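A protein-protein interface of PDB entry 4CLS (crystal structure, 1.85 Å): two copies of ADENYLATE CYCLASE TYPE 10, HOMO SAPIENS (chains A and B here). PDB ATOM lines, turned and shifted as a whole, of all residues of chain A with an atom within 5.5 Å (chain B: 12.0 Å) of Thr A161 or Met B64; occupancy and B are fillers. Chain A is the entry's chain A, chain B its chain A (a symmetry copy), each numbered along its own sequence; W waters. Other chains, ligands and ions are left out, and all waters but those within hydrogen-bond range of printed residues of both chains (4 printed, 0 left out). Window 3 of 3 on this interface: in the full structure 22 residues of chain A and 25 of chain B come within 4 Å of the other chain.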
ATOM      1  N   ASP A 159     -36.742 -32.684   8.120  1.00  0.00           N
ATOM      2  CA  ASP A 159     -36.082 -31.585   8.795  1.00  0.00           C
ATOM      3  C   ASP A 159     -35.126 -30.959   7.850  1.00  0.00           C
ATOM      4  O   ASP A 159     -35.292 -31.141   6.694  1.00  0.00           O
ATOM      5  CB  ASP A 159     -35.425 -32.037  10.093  1.00  0.00           C
ATOM      6  CG  ASP A 159     -34.348 -33.086   9.890  1.00  0.00           C
ATOM      7  OD1 ASP A 159     -33.759 -33.232   8.779  1.00  0.00           O
ATOM      8  OD2 ASP A 159     -34.083 -33.745  10.891  1.00  0.00           O
ATOM      9  N   GLU A 160     -34.142 -30.191   8.355  1.00  0.00           N
ATOM     10  CA  GLU A 160     -33.280 -29.437   7.512  1.00  0.00           C
ATOM     11  C   GLU A 160     -32.287 -30.292   6.721  1.00  0.00           C
ATOM     12  O   GLU A 160     -31.757 -29.823   5.745  1.00  0.00           O
ATOM     13  CB  GLU A 160     -32.517 -28.342   8.276  1.00  0.00           C
ATOM     14  CG  GLU A 160     -33.435 -27.400   9.074  1.00  0.00           C
ATOM     15  CD  GLU A 160     -33.632 -27.874  10.530  1.00  0.00           C
ATOM     16  OE1 GLU A 160     -33.528 -29.114  10.849  1.00  0.00           O
ATOM     17  OE2 GLU A 160     -33.861 -26.983  11.398  1.00  0.00           O
ATOM     18  N   THR A 161     -32.021 -31.521   7.160  1.00  0.00           N
ATOM     19  CA  THR A 161     -31.028 -32.372   6.493  1.00  0.00           C
ATOM     20  C   THR A 161     -31.626 -33.607   5.822  1.00  0.00           C
ATOM     21  O   THR A 161     -30.973 -34.177   4.947  1.00  0.00           O
ATOM     22  CB  THR A 161     -29.883 -32.794   7.462  1.00  0.00           C
ATOM     23  OG1 THR A 161     -30.373 -33.767   8.357  1.00  0.00           O
ATOM     24  CG2 THR A 161     -29.507 -31.671   8.281  1.00  0.00           C
ATOM     25  N   HIS A 162     -32.851 -34.003   6.204  1.00  0.00           N
ATOM     26  CA  HIS A 162     -33.501 -35.210   5.711  1.00  0.00           C
ATOM     27  C   HIS A 162     -34.911 -34.945   5.253  1.00  0.00           C
ATOM     28  O   HIS A 162     -35.655 -34.170   5.848  1.00  0.00           O
ATOM     29  CB  HIS A 162     -33.503 -36.324   6.793  1.00  0.00           C
ATOM     30  CG  HIS A 162     -32.119 -36.757   7.231  1.00  0.00           C
ATOM     31  ND1 HIS A 162     -31.649 -36.566   8.512  1.00  0.00           N
ATOM     32  CD2 HIS A 162     -31.075 -37.254   6.512  1.00  0.00           C
ATOM     33  CE1 HIS A 162     -30.386 -36.951   8.579  1.00  0.00           C
ATOM     34  NE2 HIS A 162     -30.009 -37.355   7.368  1.00  0.00           N
ATOM     35  N   SER A 163     -35.300 -35.627   4.203  1.00  0.00           N
ATOM     36  CA  SER A 163     -36.644 -35.555   3.623  1.00  0.00           C
ATOM     37  C   SER A 163     -37.161 -36.959   3.356  1.00  0.00           C
ATOM     38  O   SER A 163     -36.393 -37.843   2.983  1.00  0.00           O
ATOM     39  CB  SER A 163     -36.642 -34.762   2.313  1.00  0.00           C
ATOM     40  OG  SER A 163     -36.240 -33.435   2.558  1.00  0.00           O
ATOM     41  N   MET A 263     -28.619 -30.374  -3.482  1.00  0.00           N
ATOM     42  CA  MET A 263     -28.828 -30.220  -2.038  1.00  0.00           C
ATOM     43  C   MET A 263     -30.222 -30.659  -1.579  1.00  0.00           C
ATOM     44  O   MET A 263     -30.384 -31.279  -0.530  1.00  0.00           O
ATOM     45  CB  MET A 263     -28.573 -28.782  -1.634  1.00  0.00           C
ATOM     46  CG  MET A 263     -27.131 -28.439  -1.316  1.00  0.00           C
ATOM     47  SD  MET A 263     -27.139 -26.796  -0.588  1.00  0.00           S
ATOM     48  CE  MET A 263     -27.458 -25.775  -2.028  1.00  0.00           C
ATOM     49  N   SER A 264     -31.242 -30.355  -2.371  1.00  0.00           N
ATOM     50  CA  SER A 264     -32.581 -30.758  -2.099  1.00  0.00           C
ATOM     51  C   SER A 264     -32.801 -32.303  -2.271  1.00  0.00           C
ATOM     52  O   SER A 264     -33.358 -32.986  -1.358  1.00  0.00           O
ATOM     53  CB  SER A 264     -33.487 -29.881  -2.997  1.00  0.00           C
ATOM     54  OG  SER A 264     -34.670 -30.538  -3.120  1.00  0.00           O
ATOM     55  N   GLN A 266     -30.405 -34.780  -2.246  1.00  0.00           N
ATOM     56  CA  GLN A 266     -29.604 -35.657  -1.420  1.00  0.00           C
ATOM     57  C   GLN A 266     -30.255 -35.962  -0.060  1.00  0.00           C
ATOM     58  O   GLN A 266     -29.930 -36.986   0.570  1.00  0.00           O
ATOM     59  CB  GLN A 266     -28.207 -35.059  -1.235  1.00  0.00           C
ATOM     60  CG  GLN A 266     -28.137 -33.970  -0.205  1.00  0.00           C
ATOM     61  CD  GLN A 266     -26.760 -33.848   0.347  1.00  0.00           C
ATOM     62  OE1 GLN A 266     -25.855 -33.429  -0.342  1.00  0.00           O
ATOM     63  NE2 GLN A 266     -26.585 -34.275   1.610  1.00  0.00           N
ATOM     64  N   LYS A 267     -31.170 -35.100   0.375  1.00  0.00           N
ATOM     65  CA  LYS A 267     -31.798 -35.217   1.693  1.00  0.00           C
ATOM     66  C   LYS A 267     -32.673 -36.460   1.800  1.00  0.00           C
ATOM     67  O   LYS A 267     -32.962 -36.930   2.918  1.00  0.00           O
ATOM     68  CB  LYS A 267     -32.644 -34.014   1.998  1.00  0.00           C
ATOM     69  CG  LYS A 267     -31.818 -32.786   2.154  1.00  0.00           C
ATOM     70  CD  LYS A 267     -32.657 -31.590   2.569  1.00  0.00           C
ATOM     71  CE  LYS A 267     -31.612 -30.504   2.731  1.00  0.00           C
ATOM     72  NZ  LYS A 267     -32.267 -29.278   2.385  1.00  0.00           N
ATOM     73  N   GLU A 271     -26.798 -41.348   4.030  1.00  0.00           N
ATOM     74  CA  GLU A 271     -25.404 -40.952   3.962  1.00  0.00           C
ATOM     75  C   GLU A 271     -24.442 -42.036   3.390  1.00  0.00           C
ATOM     76  O   GLU A 271     -23.530 -41.699   2.645  1.00  0.00           O
ATOM     77  CB  GLU A 271     -24.909 -40.444   5.323  1.00  0.00           C
ATOM     78  CG  GLU A 271     -25.354 -38.993   5.594  1.00  0.00           C
ATOM     79  CD  GLU A 271     -26.815 -38.883   6.151  1.00  0.00           C
ATOM     80  OE1 GLU A 271     -27.522 -39.937   6.349  1.00  0.00           O
ATOM     81  OE2 GLU A 271     -27.257 -37.730   6.421  1.00  0.00           O
ATOM     82  N   MET B  54     -17.038 -19.220  -4.321  1.00  0.00           N
ATOM     83  CA  MET B  54     -17.942 -20.336  -4.266  1.00  0.00           C
ATOM     84  C   MET B  54     -17.326 -21.381  -3.372  1.00  0.00           C
ATOM     85  O   MET B  54     -18.008 -21.998  -2.559  1.00  0.00           O
ATOM     86  CB  MET B  54     -18.154 -20.897  -5.663  1.00  0.00           C
ATOM     87  CG  MET B  54     -19.618 -20.976  -6.033  1.00  0.00           C
ATOM     88  SD  MET B  54     -19.790 -21.969  -7.522  1.00  0.00           S
ATOM     89  CE  MET B  54     -19.379 -20.691  -8.708  1.00  0.00           C
ATOM     90  N   THR B  55     -16.011 -21.547  -3.499  1.00  0.00           N
ATOM     91  CA  THR B  55     -15.304 -22.393  -2.615  1.00  0.00           C
ATOM     92  C   THR B  55     -15.634 -22.098  -1.182  1.00  0.00           C
ATOM     93  O   THR B  55     -15.902 -23.003  -0.447  1.00  0.00           O
ATOM     94  CB  THR B  55     -13.782 -22.407  -2.889  1.00  0.00           C
ATOM     95  OG1 THR B  55     -13.572 -23.053  -4.147  1.00  0.00           O
ATOM     96  CG2 THR B  55     -13.077 -23.210  -1.873  1.00  0.00           C
ATOM     97  N   GLU B  56     -15.614 -20.843  -0.740  1.00  0.00           N
ATOM     98  CA  GLU B  56     -15.868 -20.559   0.665  1.00  0.00           C
ATOM     99  C   GLU B  56     -17.290 -20.947   1.102  1.00  0.00           C
ATOM    100  O   GLU B  56     -17.520 -21.525   2.183  1.00  0.00           O
ATOM    101  CB  GLU B  56     -15.707 -19.046   0.894  1.00  0.00           C
ATOM    102  CG  GLU B  56     -15.821 -18.641   2.341  1.00  0.00           C
ATOM    103  CD  GLU B  56     -14.480 -18.628   3.050  1.00  0.00           C
ATOM    104  OE1 GLU B  56     -13.475 -19.194   2.500  1.00  0.00           O
ATOM    105  OE2 GLU B  56     -14.440 -18.026   4.151  1.00  0.00           O
ATOM    106  N   LYS B  57     -18.231 -20.618   0.240  1.00  0.00           N
ATOM    107  CA  LYS B  57     -19.598 -20.969   0.440  1.00  0.00           C
ATOM    108  C   LYS B  57     -19.868 -22.484   0.536  1.00  0.00           C
ATOM    109  O   LYS B  57     -20.788 -22.904   1.215  1.00  0.00           O
ATOM    110  CB  LYS B  57     -20.339 -20.424  -0.770  1.00  0.00           C
ATOM    111  CG  LYS B  57     -21.806 -20.765  -0.869  1.00  0.00           C
ATOM    112  CD  LYS B  57     -22.432 -19.937  -2.002  1.00  0.00           C
ATOM    113  CE  LYS B  57     -23.938 -20.150  -2.124  1.00  0.00           C
ATOM    114  NZ  LYS B  57     -24.572 -20.267  -0.771  1.00  0.00           N
ATOM    115  N   PHE B  58     -19.073 -23.303  -0.163  1.00  0.00           N
ATOM    116  CA  PHE B  58     -19.308 -24.763  -0.167  1.00  0.00           C
ATOM    117  C   PHE B  58     -18.877 -25.379   1.129  1.00  0.00           C
ATOM    118  O   PHE B  58     -19.270 -26.527   1.407  1.00  0.00           O
ATOM    119  CB  PHE B  58     -18.633 -25.455  -1.348  1.00  0.00           C
ATOM    120  CG  PHE B  58     -19.402 -25.335  -2.631  1.00  0.00           C
ATOM    121  CD1 PHE B  58     -20.438 -26.165  -2.905  1.00  0.00           C
ATOM    122  CD2 PHE B  58     -19.046 -24.411  -3.587  1.00  0.00           C
ATOM    123  CE1 PHE B  58     -21.163 -26.062  -4.061  1.00  0.00           C
ATOM    124  CE2 PHE B  58     -19.746 -24.317  -4.789  1.00  0.00           C
ATOM    125  CZ  PHE B  58     -20.821 -25.147  -5.023  1.00  0.00           C
ATOM    126  N   SER B  59     -18.123 -24.617   1.961  1.00  0.00           N
ATOM    127  CA  SER B  59     -17.886 -25.017   3.358  1.00  0.00           C
ATOM    128  C   SER B  59     -19.048 -24.835   4.350  1.00  0.00           C
ATOM    129  O   SER B  59     -19.017 -25.336   5.481  1.00  0.00           O
ATOM    130  CB  SER B  59     -16.685 -24.272   3.895  1.00  0.00           C
ATOM    131  OG  SER B  59     -15.543 -25.053   3.618  1.00  0.00           O
ATOM    132  N   SER B  60     -20.106 -24.161   3.947  1.00  0.00           N
ATOM    133  CA  SER B  60     -21.157 -23.872   4.902  1.00  0.00           C
ATOM    134  C   SER B  60     -22.018 -25.113   5.144  1.00  0.00           C
ATOM    135  O   SER B  60     -22.073 -26.071   4.304  1.00  0.00           O
ATOM    136  CB  SER B  60     -21.991 -22.743   4.358  1.00  0.00           C
ATOM    137  OG  SER B  60     -22.945 -23.217   3.474  1.00  0.00           O
ATOM    138  N   ALA B  61     -22.691 -25.084   6.287  1.00  0.00           N
ATOM    139  CA  ALA B  61     -23.534 -26.147   6.727  1.00  0.00           C
ATOM    140  C   ALA B  61     -24.569 -26.500   5.692  1.00  0.00           C
ATOM    141  O   ALA B  61     -25.095 -27.610   5.738  1.00  0.00           O
ATOM    142  CB  ALA B  61     -24.224 -25.756   8.034  1.00  0.00           C
ATOM    143  N   MET B  62     -24.919 -25.594   4.765  1.00  0.00           N
ATOM    144  CA  MET B  62     -26.017 -25.967   3.852  1.00  0.00           C
ATOM    145  C   MET B  62     -25.649 -27.116   2.952  1.00  0.00           C
ATOM    146  O   MET B  62     -26.541 -27.859   2.498  1.00  0.00           O
ATOM    147  CB  MET B  62     -26.592 -24.806   3.056  1.00  0.00           C
ATOM    148  CG  MET B  62     -25.634 -24.082   2.178  1.00  0.00           C
ATOM    149  SD  MET B  62     -26.523 -22.893   1.111  1.00  0.00           S
ATOM    150  CE  MET B  62     -27.252 -21.896   2.424  1.00  0.00           C
ATOM    151  N   TYR B  63     -24.358 -27.295   2.717  1.00  0.00           N
ATOM    152  CA  TYR B  63     -23.913 -28.378   1.843  1.00  0.00           C
ATOM    153  C   TYR B  63     -23.733 -29.749   2.528  1.00  0.00           C
ATOM    154  O   TYR B  63     -23.353 -30.770   1.863  1.00  0.00           O
ATOM    155  CB  TYR B  63     -22.657 -27.964   1.073  1.00  0.00           C
ATOM    156  CG  TYR B  63     -23.032 -26.917   0.063  1.00  0.00           C
ATOM    157  CD1 TYR B  63     -23.520 -27.293  -1.195  1.00  0.00           C
ATOM    158  CD2 TYR B  63     -22.899 -25.544   0.361  1.00  0.00           C
ATOM    159  CE1 TYR B  63     -23.893 -26.333  -2.117  1.00  0.00           C
ATOM    160  CE2 TYR B  63     -23.245 -24.584  -0.566  1.00  0.00           C
ATOM    161  CZ  TYR B  63     -23.737 -24.989  -1.797  1.00  0.00           C
ATOM    162  OH  TYR B  63     -24.106 -24.080  -2.734  1.00  0.00           O
ATOM    163  N   MET B  64     -23.997 -29.760   3.841  1.00  0.00           N
ATOM    164  CA  MET B  64     -24.178 -30.995   4.601  1.00  0.00           C
ATOM    165  C   MET B  64     -22.934 -31.881   4.426  1.00  0.00           C
ATOM    166  O   MET B  64     -23.060 -33.062   4.156  1.00  0.00           O
ATOM    167  CB  MET B  64     -25.438 -31.738   4.139  1.00  0.00           C
ATOM    168  CG  MET B  64     -26.719 -30.977   4.518  1.00  0.00           C
ATOM    169  SD  MET B  64     -28.210 -31.572   3.718  1.00  0.00           S
ATOM    170  CE  MET B  64     -28.075 -30.998   2.005  1.00  0.00           C
ATOM    171  N   ASP B  65     -21.760 -31.317   4.567  1.00  0.00           N
ATOM    172  CA  ASP B  65     -20.521 -32.115   4.458  1.00  0.00           C
ATOM    173  C   ASP B  65     -20.275 -32.760   3.087  1.00  0.00           C
ATOM    174  O   ASP B  65     -19.364 -33.599   2.992  1.00  0.00           O
ATOM    175  CB  ASP B  65     -20.440 -33.228   5.491  1.00  0.00           C
ATOM    176  CG  ASP B  65     -20.638 -32.687   6.870  1.00  0.00           C
ATOM    177  OD1 ASP B  65     -19.982 -31.690   7.175  1.00  0.00           O
ATOM    178  OD2 ASP B  65     -21.509 -33.197   7.571  1.00  0.00           O
ATOM    179  N   ARG B  66     -21.023 -32.354   2.050  1.00  0.00           N
ATOM    180  CA  ARG B  66     -20.664 -32.782   0.718  1.00  0.00           C
ATOM    181  C   ARG B  66     -20.231 -31.559  -0.095  1.00  0.00           C
ATOM    182  O   ARG B  66     -20.304 -31.578  -1.310  1.00  0.00           O
ATOM    183  CB  ARG B  66     -21.856 -33.481   0.008  1.00  0.00           C
ATOM    184  CG  ARG B  66     -22.065 -34.923   0.571  1.00  0.00           C
ATOM    185  CD  ARG B  66     -23.143 -35.688  -0.158  1.00  0.00           C
ATOM    186  NE  ARG B  66     -22.741 -35.955  -1.519  1.00  0.00           N
ATOM    187  CZ  ARG B  66     -23.187 -35.352  -2.600  1.00  0.00           C
ATOM    188  NH1 ARG B  66     -24.125 -34.441  -2.525  1.00  0.00           N
ATOM    189  NH2 ARG B  66     -22.673 -35.682  -3.780  1.00  0.00           N
ATOM    190  N   GLY B  67     -19.708 -30.531   0.560  1.00  0.00           N
ATOM    191  CA  GLY B  67     -19.161 -29.423  -0.196  1.00  0.00           C
ATOM    192  C   GLY B  67     -18.149 -29.697  -1.239  1.00  0.00           C
ATOM    193  O   GLY B  67     -18.219 -29.145  -2.347  1.00  0.00           O
ATOM    194  N   ALA B  68     -17.121 -30.464  -0.910  1.00  0.00           N
ATOM    195  CA  ALA B  68     -16.128 -30.761  -1.889  1.00  0.00           C
ATOM    196  C   ALA B  68     -16.648 -31.484  -3.101  1.00  0.00           C
ATOM    197  O   ALA B  68     -16.242 -31.187  -4.231  1.00  0.00           O
ATOM    198  CB  ALA B  68     -14.970 -31.564  -1.286  1.00  0.00           C
ATOM    199  N   GLU B  69     -17.561 -32.410  -2.854  1.00  0.00           N
ATOM    200  CA  GLU B  69     -18.140 -33.228  -3.945  1.00  0.00           C
ATOM    201  C   GLU B  69     -19.012 -32.379  -4.844  1.00  0.00           C
ATOM    202  O   GLU B  69     -18.934 -32.427  -6.102  1.00  0.00           O
ATOM    203  CB  GLU B  69     -18.948 -34.345  -3.284  1.00  0.00           C
ATOM    204  CG  GLU B  69     -18.030 -35.362  -2.609  1.00  0.00           C
ATOM    205  CD  GLU B  69     -17.614 -35.020  -1.203  1.00  0.00           C
ATOM    206  OE1 GLU B  69     -18.045 -33.978  -0.599  1.00  0.00           O
ATOM    207  OE2 GLU B  69     -16.843 -35.837  -0.654  1.00  0.00           O
ATOM    208  N   GLN B  70     -19.805 -31.512  -4.212  1.00  0.00           N
ATOM    209  CA  GLN B  70     -20.621 -30.587  -5.030  1.00  0.00           C
ATOM    210  C   GLN B  70     -19.775 -29.562  -5.805  1.00  0.00           C
ATOM    211  O   GLN B  70     -20.066 -29.225  -6.975  1.00  0.00           O
ATOM    212  CB  GLN B  70     -21.563 -29.857  -4.077  1.00  0.00           C
ATOM    213  CG  GLN B  70     -22.717 -30.736  -3.644  1.00  0.00           C
ATOM    214  CD  GLN B  70     -24.042 -30.248  -4.135  1.00  0.00           C
ATOM    215  OE1 GLN B  70     -24.217 -29.934  -5.322  1.00  0.00           O
ATOM    216  NE2 GLN B  70     -24.992 -30.212  -3.252  1.00  0.00           N
ATOM    217  N   LEU B  71     -18.690 -29.064  -5.177  1.00  0.00           N
ATOM    218  CA  LEU B  71     -17.885 -28.050  -5.824  1.00  0.00           C
ATOM    219  C   LEU B  71     -17.186 -28.623  -7.055  1.00  0.00           C
ATOM    220  O   LEU B  71     -17.226 -28.009  -8.160  1.00  0.00           O
ATOM    221  CB  LEU B  71     -16.886 -27.456  -4.849  1.00  0.00           C
ATOM    222  CG  LEU B  71     -15.924 -26.434  -5.469  1.00  0.00           C
ATOM    223  CD1 LEU B  71     -16.670 -25.132  -5.757  1.00  0.00           C
ATOM    224  CD2 LEU B  71     -14.740 -26.215  -4.556  1.00  0.00           C
ATOM    225  N   GLU B  73     -18.014 -31.161  -8.792  1.00  0.00           N
ATOM    226  CA  GLU B  73     -19.025 -31.484  -9.822  1.00  0.00           C
ATOM    227  C   GLU B  73     -19.400 -30.256 -10.666  1.00  0.00           C
ATOM    228  O   GLU B  73     -19.399 -30.329 -11.901  1.00  0.00           O
ATOM    229  CB  GLU B  73     -20.260 -32.061  -9.106  1.00  0.00           C
ATOM    230  CG  GLU B  73     -21.358 -32.465 -10.068  1.00  0.00           C
ATOM    231  CD  GLU B  73     -22.555 -33.030  -9.314  1.00  0.00           C
ATOM    232  OE1 GLU B  73     -22.640 -32.828  -8.064  1.00  0.00           O
ATOM    233  OE2 GLU B  73     -23.374 -33.607 -10.003  1.00  0.00           O
ATOM    234  N   SER B 287     -10.927 -35.690  -3.752  1.00  0.00           N
ATOM    235  CA  SER B 287     -11.747 -34.471  -3.737  1.00  0.00           C
ATOM    236  C   SER B 287     -12.055 -34.159  -2.317  1.00  0.00           C
ATOM    237  O   SER B 287     -12.796 -34.910  -1.689  1.00  0.00           O
ATOM    238  CB  SER B 287     -13.086 -34.659  -4.465  1.00  0.00           C
ATOM    239  OG  SER B 287     -12.858 -34.777  -5.846  1.00  0.00           O
ATOM    240  N   LEU B 289     -12.282 -30.870   0.975  1.00  0.00           N
ATOM    241  CA  LEU B 289     -12.102 -29.526   1.493  1.00  0.00           C
ATOM    242  C   LEU B 289     -11.369 -29.819   2.785  1.00  0.00           C
ATOM    243  O   LEU B 289     -11.872 -30.517   3.639  1.00  0.00           O
ATOM    244  CB  LEU B 289     -13.471 -28.865   1.811  1.00  0.00           C
ATOM    245  CG  LEU B 289     -14.157 -28.184   0.641  1.00  0.00           C
ATOM    246  CD1 LEU B 289     -15.578 -27.793   1.034  1.00  0.00           C
ATOM    247  CD2 LEU B 289     -13.486 -26.887   0.157  1.00  0.00           C
HETATM  248  O   HOH W   1     -24.799 -30.881  -0.523  1.00  0.00           O
HETATM  249  O   HOH W   2     -24.458 -35.179   3.378  1.00  0.00           O
HETATM  250  O   HOH W   3     -28.676 -35.052   3.643  1.00  0.00           O
HETATM  251  O   HOH W   4     -29.224 -27.594   2.514  1.00  0.00           O
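NE2 of Gln A266 lies close to SD of Met B64 (3.8 Å).
The side-chain amide oxygen of Gln A266 is in hydrogen-bond range of the guanidinium group of Arg B66 (3.0 Å).
SD of Met A263 lies close to O of Met B62.
The side-chain carboxylate of Asp A159 is in hydrogen-bond range of the backbone NH of Thr A161 (2.9 Å).
The side-chain amino group (NZ) of Lys A267 lies close to the backbone carbonyl oxygen (O) of Glu A160.
A ring nitrogen (ND1) of His A162 sits at hydrogen-bond distance from the side-chain hydroxyl (OG1) of Thr A161.
The backbone carbonyl oxygen (O) of Lys A267 sits at hydrogen-bond distance from the backbone NH (N) of Ser A163 (3.0 Å).
The side-chain amino group (NZ) of Lys B57 sits at hydrogen-bond distance from the side-chain sulfur (SD) of Met B62, 3.8 Å away.
OG of Ser B60 sits close to N of Met B62 (3.3 Å).
Among the printed residues, pairs that only touch across the chains: Thr A161 with Met B64 (3.99 Å), Met A263 with Tyr B63 (3.6 Å), Met A263 with Met B64 (3.4 Å), Met A263 with Gln B70 (3.4 Å) and Lys A267 with Met B64 (3.6 Å).
No residue of chain B comes within 4 Å of Asp A159.
No residue of chain B comes within 4 Å of Glu A160.
Of the printed residues of chain B, Thr A161 touches Met B64.
No residue of chain B comes within 4 Å of His A162.
No residue of chain B comes within 4 Å of Ser A163.
Of the printed residues of chain B, Met A263 touches Met B62, Tyr B63, Met B64 and Gln B70.
Of the printed residues of chain B, Gln A266 touches Met B64 and Arg B66.
Of the printed residues of chain B, Lys A267 touches Met B64.
Lys B57 touches none of the printed residues of chain A.
Printed residues of chain A within 4 Å of Tyr B63: Met A263 (3.6 Å).
Printed residues of chain A within 4 Å of Met B64: Thr A161, Met A263, Gln A266 and Lys A267.
Glu B69 touches none of the printed residues of chain A.
Of the printed residues of chain A, Gln B70 touches Met A263 (3.4 Å).
The nearest printed residue of chain A that does not touch Met B64 is Glu A160 (4.4 Å).
The nearest printed residue of chain A that does not touch Arg B66 is Met A263 (6.1 Å).
Of the 21 printed residues of chain B, 5 touch a printed residue of chain A.
Hydrophobic or aromatic side chains of chain B that line the printed part of chain A: Tyr B63 and Met B64.
Hydrophobic or aromatic side chains of chain A that line the printed part of chain B: Met A263.
Among the printed residues, 8 pairs touch across the chains.
Among the printed residues, no Asp or Glu carboxylate lies within 4 Å of a Lys or Arg side-chain nitrogen of the other chain.
No position is printed for both chains.
Of the 8 pairs that touch across the chains among the printed residues, none has its exchanged pair printed and touching as well.
Water W2 bridges the backbone carbonyl oxygen of Met B64 (2.7 Å) and the side-chain amide nitrogen of Gln A266 (2.9 Å).
Water W4 lies within hydrogen-bond range of the backbone carbonyl oxygen of Met B62 (2.7 Å) and the side-chain amino group of Lys A267 (3.5 Å).
Water W1 lies within hydrogen-bond range of the side-chain amide oxygen of Gln A266 (2.8 Å), the backbone carbonyl oxygen of Tyr B63 (2.8 Å) and the side-chain amide nitrogen of Gln B70 (2.8 Å).
Water W3 lies within hydrogen-bond range of O of Thr A161, NE2 of Gln A266 and SD of Met B64.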
